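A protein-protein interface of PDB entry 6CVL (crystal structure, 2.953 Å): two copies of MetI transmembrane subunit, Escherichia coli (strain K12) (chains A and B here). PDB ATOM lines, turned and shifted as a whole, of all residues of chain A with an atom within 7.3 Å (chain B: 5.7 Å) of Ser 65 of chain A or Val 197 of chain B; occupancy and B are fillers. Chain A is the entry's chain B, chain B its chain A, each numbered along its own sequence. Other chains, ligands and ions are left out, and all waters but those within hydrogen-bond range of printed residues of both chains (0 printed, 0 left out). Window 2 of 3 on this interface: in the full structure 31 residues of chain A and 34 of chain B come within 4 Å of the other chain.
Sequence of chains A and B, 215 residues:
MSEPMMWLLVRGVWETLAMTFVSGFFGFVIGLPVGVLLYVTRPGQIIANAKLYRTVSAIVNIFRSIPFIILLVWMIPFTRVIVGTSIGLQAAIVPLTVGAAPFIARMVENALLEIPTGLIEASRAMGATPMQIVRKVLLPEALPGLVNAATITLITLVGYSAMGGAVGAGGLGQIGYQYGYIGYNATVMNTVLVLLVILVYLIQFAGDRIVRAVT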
ATOM      1  N   ALA A  58      35.438 -28.977  14.626  1.00  0.00           N
ATOM      2  CA  ALA A  58      34.360 -29.945  14.513  1.00  0.00           C
ATOM      3  C   ALA A  58      33.708 -30.174  15.863  1.00  0.00           C
ATOM      4  O   ALA A  58      32.482 -30.150  15.984  1.00  0.00           O
ATOM      5  CB  ALA A  58      34.904 -31.256  13.950  1.00  0.00           C
ATOM      6  N   ILE A  59      34.519 -30.420  16.889  1.00  0.00           N
ATOM      7  CA  ILE A  59      33.981 -30.583  18.234  1.00  0.00           C
ATOM      8  C   ILE A  59      33.133 -29.374  18.596  1.00  0.00           C
ATOM      9  O   ILE A  59      32.004 -29.495  19.094  1.00  0.00           O
ATOM     10  CB  ILE A  59      35.124 -30.790  19.242  1.00  0.00           C
ATOM     11  CG1 ILE A  59      35.715 -32.192  19.080  1.00  0.00           C
ATOM     12  CG2 ILE A  59      34.627 -30.555  20.660  1.00  0.00           C
ATOM     13  CD1 ILE A  59      36.965 -32.439  19.908  1.00  0.00           C
ATOM     14  N   VAL A  60      33.675 -28.185  18.351  1.00  0.00           N
ATOM     15  CA  VAL A  60      33.000 -26.956  18.744  1.00  0.00           C
ATOM     16  C   VAL A  60      31.653 -26.852  18.047  1.00  0.00           C
ATOM     17  O   VAL A  60      30.620 -26.624  18.685  1.00  0.00           O
ATOM     18  CB  VAL A  60      33.900 -25.747  18.433  1.00  0.00           C
ATOM     19  CG1 VAL A  60      33.104 -24.453  18.462  1.00  0.00           C
ATOM     20  CG2 VAL A  60      35.058 -25.700  19.418  1.00  0.00           C
ATOM     21  N   ASN A  61      31.642 -27.042  16.731  1.00  0.00           N
ATOM     22  CA  ASN A  61      30.401 -26.928  15.974  1.00  0.00           C
ATOM     23  C   ASN A  61      29.407 -28.000  16.395  1.00  0.00           C
ATOM     24  O   ASN A  61      28.203 -27.735  16.504  1.00  0.00           O
ATOM     25  CB  ASN A  61      30.697 -27.026  14.479  1.00  0.00           C
ATOM     26  CG  ASN A  61      31.811 -26.093  14.043  1.00  0.00           C
ATOM     27  OD1 ASN A  61      31.871 -24.937  14.465  1.00  0.00           O
ATOM     28  ND2 ASN A  61      32.708 -26.595  13.206  1.00  0.00           N
ATOM     29  N   ILE A  62      29.893 -29.217  16.637  1.00  0.00           N
ATOM     30  CA  ILE A  62      29.018 -30.301  17.055  1.00  0.00           C
ATOM     31  C   ILE A  62      28.299 -29.922  18.336  1.00  0.00           C
ATOM     32  O   ILE A  62      27.069 -29.995  18.427  1.00  0.00           O
ATOM     33  CB  ILE A  62      29.825 -31.598  17.237  1.00  0.00           C
ATOM     34  CG1 ILE A  62      30.233 -32.169  15.880  1.00  0.00           C
ATOM     35  CG2 ILE A  62      29.020 -32.618  18.037  1.00  0.00           C
ATOM     36  CD1 ILE A  62      31.405 -33.128  15.957  1.00  0.00           C
ATOM     37  N   PHE A  63      29.058 -29.503  19.346  1.00  0.00           N
ATOM     38  CA  PHE A  63      28.428 -29.119  20.603  1.00  0.00           C
ATOM     39  C   PHE A  63      27.492 -27.938  20.399  1.00  0.00           C
ATOM     40  O   PHE A  63      26.419 -27.874  21.008  1.00  0.00           O
ATOM     41  CB  PHE A  63      29.488 -28.806  21.655  1.00  0.00           C
ATOM     42  CG  PHE A  63      29.919 -30.011  22.440  1.00  0.00           C
ATOM     43  CD1 PHE A  63      29.170 -30.452  23.517  1.00  0.00           C
ATOM     44  CD2 PHE A  63      31.071 -30.703  22.105  1.00  0.00           C
ATOM     45  CE1 PHE A  63      29.558 -31.561  24.242  1.00  0.00           C
ATOM     46  CE2 PHE A  63      31.464 -31.813  22.832  1.00  0.00           C
ATOM     47  CZ  PHE A  63      30.704 -32.240  23.901  1.00  0.00           C
ATOM     48  N   ARG A  64      27.867 -27.002  19.528  1.00  0.00           N
ATOM     49  CA  ARG A  64      26.992 -25.872  19.250  1.00  0.00           C
ATOM     50  C   ARG A  64      25.657 -26.323  18.668  1.00  0.00           C
ATOM     51  O   ARG A  64      24.627 -25.691  18.923  1.00  0.00           O
ATOM     52  CB  ARG A  64      27.693 -24.899  18.300  1.00  0.00           C
ATOM     53  CG  ARG A  64      28.910 -24.209  18.910  1.00  0.00           C
ATOM     54  CD  ARG A  64      28.594 -22.800  19.393  1.00  0.00           C
ATOM     55  NE  ARG A  64      28.908 -21.783  18.388  1.00  0.00           N
ATOM     56  CZ  ARG A  64      28.445 -20.535  18.411  1.00  0.00           C
ATOM     57  NH1 ARG A  64      27.636 -20.137  19.383  1.00  0.00           N
ATOM     58  NH2 ARG A  64      28.790 -19.679  17.459  1.00  0.00           N
ATOM     59  N   SER A  65      25.651 -27.402  17.885  1.00  0.00           N
ATOM     60  CA  SER A  65      24.450 -27.829  17.175  1.00  0.00           C
ATOM     61  C   SER A  65      23.465 -28.630  18.025  1.00  0.00           C
ATOM     62  O   SER A  65      22.366 -28.924  17.542  1.00  0.00           O
ATOM     63  CB  SER A  65      24.847 -28.652  15.948  1.00  0.00           C
ATOM     64  OG  SER A  65      25.855 -29.588  16.279  1.00  0.00           O
ATOM     65  N   ILE A  66      23.822 -29.017  19.243  1.00  0.00           N
ATOM     66  CA  ILE A  66      22.892 -29.761  20.100  1.00  0.00           C
ATOM     67  C   ILE A  66      21.948 -28.774  20.782  1.00  0.00           C
ATOM     68  O   ILE A  66      22.418 -27.785  21.367  1.00  0.00           O
ATOM     69  CB  ILE A  66      23.646 -30.588  21.134  1.00  0.00           C
ATOM     70  CG1 ILE A  66      24.616 -31.558  20.461  1.00  0.00           C
ATOM     71  CG2 ILE A  66      22.652 -31.346  22.004  1.00  0.00           C
ATOM     72  CD1 ILE A  66      25.585 -32.202  21.428  1.00  0.00           C
ATOM     73  N   PRO A  67      20.633 -28.994  20.735  1.00  0.00           N
ATOM     74  CA  PRO A  67      19.729 -28.164  21.536  1.00  0.00           C
ATOM     75  C   PRO A  67      20.054 -28.250  23.018  1.00  0.00           C
ATOM     76  O   PRO A  67      20.598 -29.246  23.504  1.00  0.00           O
ATOM     77  CB  PRO A  67      18.347 -28.750  21.231  1.00  0.00           C
ATOM     78  CG  PRO A  67      18.488 -29.321  19.871  1.00  0.00           C
ATOM     79  CD  PRO A  67      19.891 -29.865  19.806  1.00  0.00           C
ATOM     80  N   PHE A  68      19.703 -27.183  23.741  1.00  0.00           N
ATOM     81  CA  PHE A  68      20.025 -27.111  25.162  1.00  0.00           C
ATOM     82  C   PHE A  68      19.481 -28.324  25.903  1.00  0.00           C
ATOM     83  O   PHE A  68      20.164 -28.916  26.750  1.00  0.00           O
ATOM     84  CB  PHE A  68      19.445 -25.832  25.783  1.00  0.00           C
ATOM     85  CG  PHE A  68      19.363 -24.658  24.837  1.00  0.00           C
ATOM     86  CD1 PHE A  68      20.473 -24.229  24.129  1.00  0.00           C
ATOM     87  CD2 PHE A  68      18.161 -23.990  24.653  1.00  0.00           C
ATOM     88  CE1 PHE A  68      20.385 -23.149  23.262  1.00  0.00           C
ATOM     89  CE2 PHE A  68      18.070 -22.912  23.789  1.00  0.00           C
ATOM     90  CZ  PHE A  68      19.183 -22.493  23.094  1.00  0.00           C
ATOM     91  N   VAL B 192      17.455 -35.229  13.503  1.00  0.00           N
ATOM     92  CA  VAL B 192      17.447 -33.826  13.902  1.00  0.00           C
ATOM     93  C   VAL B 192      18.866 -33.357  14.192  1.00  0.00           C
ATOM     94  O   VAL B 192      19.299 -32.294  13.728  1.00  0.00           O
ATOM     95  CB  VAL B 192      16.526 -33.617  15.116  1.00  0.00           C
ATOM     96  CG1 VAL B 192      16.806 -32.276  15.775  1.00  0.00           C
ATOM     97  CG2 VAL B 192      15.071 -33.704  14.694  1.00  0.00           C
ATOM     98  N   LEU B 193      19.606 -34.139  14.980  1.00  0.00           N
ATOM     99  CA  LEU B 193      20.962 -33.745  15.341  1.00  0.00           C
ATOM    100  C   LEU B 193      21.832 -33.594  14.103  1.00  0.00           C
ATOM    101  O   LEU B 193      22.610 -32.639  13.990  1.00  0.00           O
ATOM    102  CB  LEU B 193      21.575 -34.772  16.293  1.00  0.00           C
ATOM    103  CG  LEU B 193      20.896 -34.976  17.649  1.00  0.00           C
ATOM    104  CD1 LEU B 193      21.808 -35.749  18.595  1.00  0.00           C
ATOM    105  CD2 LEU B 193      20.482 -33.649  18.265  1.00  0.00           C
ATOM    106  N   VAL B 194      21.714 -34.530  13.161  1.00  0.00           N
ATOM    107  CA  VAL B 194      22.530 -34.481  11.955  1.00  0.00           C
ATOM    108  C   VAL B 194      22.187 -33.246  11.138  1.00  0.00           C
ATOM    109  O   VAL B 194      23.075 -32.559  10.619  1.00  0.00           O
ATOM    110  CB  VAL B 194      22.344 -35.775  11.144  1.00  0.00           C
ATOM    111  CG1 VAL B 194      23.000 -35.651   9.782  1.00  0.00           C
ATOM    112  CG2 VAL B 194      22.911 -36.964  11.910  1.00  0.00           C
ATOM    113  N   LEU B 195      20.897 -32.942  11.008  1.00  0.00           N
ATOM    114  CA  LEU B 195      20.503 -31.749  10.271  1.00  0.00           C
ATOM    115  C   LEU B 195      21.065 -30.498  10.927  1.00  0.00           C
ATOM    116  O   LEU B 195      21.570 -29.601  10.244  1.00  0.00           O
ATOM    117  CB  LEU B 195      18.983 -31.663  10.178  1.00  0.00           C
ATOM    118  CG  LEU B 195      18.325 -32.668   9.232  1.00  0.00           C
ATOM    119  CD1 LEU B 195      16.811 -32.559   9.310  1.00  0.00           C
ATOM    120  CD2 LEU B 195      18.807 -32.457   7.809  1.00  0.00           C
ATOM    121  N   LEU B 196      20.993 -30.423  12.255  1.00  0.00           N
ATOM    122  CA  LEU B 196      21.504 -29.247  12.948  1.00  0.00           C
ATOM    123  C   LEU B 196      23.010 -29.115  12.762  1.00  0.00           C
ATOM    124  O   LEU B 196      23.528 -28.008  12.562  1.00  0.00           O
ATOM    125  CB  LEU B 196      21.148 -29.326  14.431  1.00  0.00           C
ATOM    126  CG  LEU B 196      19.649 -29.324  14.737  1.00  0.00           C
ATOM    127  CD1 LEU B 196      19.416 -29.592  16.215  1.00  0.00           C
ATOM    128  CD2 LEU B 196      18.999 -28.014  14.313  1.00  0.00           C
ATOM    129  N   VAL B 197      23.730 -30.234  12.828  1.00  0.00           N
ATOM    130  CA  VAL B 197      25.174 -30.197  12.625  1.00  0.00           C
ATOM    131  C   VAL B 197      25.497 -29.728  11.215  1.00  0.00           C
ATOM    132  O   VAL B 197      26.399 -28.910  11.007  1.00  0.00           O
ATOM    133  CB  VAL B 197      25.792 -31.576  12.910  1.00  0.00           C
ATOM    134  CG1 VAL B 197      27.254 -31.581  12.514  1.00  0.00           C
ATOM    135  CG2 VAL B 197      25.634 -31.936  14.373  1.00  0.00           C
ATOM    136  N   ILE B 198      24.780 -30.252  10.222  1.00  0.00           N
ATOM    137  CA  ILE B 198      25.002 -29.828   8.845  1.00  0.00           C
ATOM    138  C   ILE B 198      24.762 -28.332   8.716  1.00  0.00           C
ATOM    139  O   ILE B 198      25.529 -27.614   8.061  1.00  0.00           O
ATOM    140  CB  ILE B 198      24.096 -30.632   7.895  1.00  0.00           C
ATOM    141  CG1 ILE B 198      24.538 -32.095   7.858  1.00  0.00           C
ATOM    142  CG2 ILE B 198      24.119 -30.031   6.495  1.00  0.00           C
ATOM    143  CD1 ILE B 198      23.547 -33.013   7.180  1.00  0.00           C
ATOM    144  N   LEU B 199      23.702 -27.840   9.351  1.00  0.00           N
ATOM    145  CA  LEU B 199      23.370 -26.422   9.272  1.00  0.00           C
ATOM    146  C   LEU B 199      24.488 -25.566   9.859  1.00  0.00           C
ATOM    147  O   LEU B 199      24.956 -24.610   9.225  1.00  0.00           O
ATOM    148  CB  LEU B 199      22.046 -26.182   9.998  1.00  0.00           C
ATOM    149  CG  LEU B 199      21.481 -24.767  10.074  1.00  0.00           C
ATOM    150  CD1 LEU B 199      21.650 -24.039   8.756  1.00  0.00           C
ATOM    151  CD2 LEU B 199      20.008 -24.837  10.465  1.00  0.00           C
ATOM    152  N   VAL B 200      24.931 -25.897  11.072  1.00  0.00           N
ATOM    153  CA  VAL B 200      25.984 -25.107  11.700  1.00  0.00           C
ATOM    154  C   VAL B 200      27.267 -25.185  10.884  1.00  0.00           C
ATOM    155  O   VAL B 200      28.000 -24.198  10.759  1.00  0.00           O
ATOM    156  CB  VAL B 200      26.216 -25.557  13.155  1.00  0.00           C
ATOM    157  CG1 VAL B 200      24.961 -25.342  13.983  1.00  0.00           C
ATOM    158  CG2 VAL B 200      26.654 -27.006  13.212  1.00  0.00           C
ATOM    159  N   TYR B 201      27.575 -26.360  10.332  1.00  0.00           N
ATOM    160  CA  TYR B 201      28.790 -26.491   9.540  1.00  0.00           C
ATOM    161  C   TYR B 201      28.728 -25.606   8.310  1.00  0.00           C
ATOM    162  O   TYR B 201      29.701 -24.928   7.973  1.00  0.00           O
ATOM    163  CB  TYR B 201      29.011 -27.943   9.139  1.00  0.00           C
ATOM    164  CG  TYR B 201      30.190 -28.560   9.836  1.00  0.00           C
ATOM    165  CD1 TYR B 201      31.475 -28.393   9.340  1.00  0.00           C
ATOM    166  CD2 TYR B 201      30.024 -29.304  10.990  1.00  0.00           C
ATOM    167  CE1 TYR B 201      32.557 -28.951   9.976  1.00  0.00           C
ATOM    168  CE2 TYR B 201      31.102 -29.866  11.631  1.00  0.00           C
ATOM    169  CZ  TYR B 201      32.362 -29.684  11.118  1.00  0.00           C
ATOM    170  OH  TYR B 201      33.439 -30.241  11.749  1.00  0.00           O
ATOM    171  N   LEU B 202      27.585 -25.596   7.630  1.00  0.00           N
ATOM    172  CA  LEU B 202      27.424 -24.724   6.477  1.00  0.00           C
ATOM    173  C   LEU B 202      27.612 -23.269   6.875  1.00  0.00           C
ATOM    174  O   LEU B 202      28.314 -22.513   6.192  1.00  0.00           O
ATOM    175  CB  LEU B 202      26.046 -24.945   5.862  1.00  0.00           C
ATOM    176  CG  LEU B 202      25.894 -26.311   5.195  1.00  0.00           C
ATOM    177  CD1 LEU B 202      24.433 -26.703   5.077  1.00  0.00           C
ATOM    178  CD2 LEU B 202      26.562 -26.292   3.830  1.00  0.00           C
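OG of Ser 65 of chain A lies within hydrogen-bond range of O of Asn 61 of chain A (3.0 Å).
The backbone carbonyl oxygen (O) of Ile 62 of chain A lies within hydrogen-bond range of the side-chain hydroxyl (OG) of Ser 65 of chain A, 2.5 Å away.
Val 197 of chain B touches just one residue of chain A: Ser 65 (3.0 Å).
Printed residues of chain B within 4 Å of Pro 67 of chain A: Leu 196.
Of the printed residues of chain B, Asn 61 of chain A touches Val 200 and Tyr 201.
Of the printed residues of chain A, Tyr 201 of chain B touches Ala 58 (2.8 Å) and Asn 61 (3.7 Å).
Ile 66 of chain A touches none of the printed residues of chain B.
Leu 193 of chain B touches none of the printed residues of chain A.
The nearest printed residue of chain A that does not touch Leu 196 of chain B is Ile 66 of chain A (5.2 Å).
No position is printed for both chains.
Among the printed residues, merely in contact across the chains: Ala 58 of chain A with Tyr 201 of chain B (2.8 Å), Asn 61 of chain A with Val 200 of chain B (3.7 Å), Asn 61 of chain A with Tyr 201 of chain B (3.7 Å), Ser 65 of chain A with Leu 196 of chain B (3.3 Å), Ser 65 of chain A with Val 197 of chain B (3.0 Å), Ser 65 of chain A with Val 200 of chain B (3.7 Å) and Pro 67 of chain A with Leu 196 of chain B (3.6 Å).
Printed residues of chain A that touch a printed residue of chain B: Ala 58, Asn 61, Ser 65 and Pro 67.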
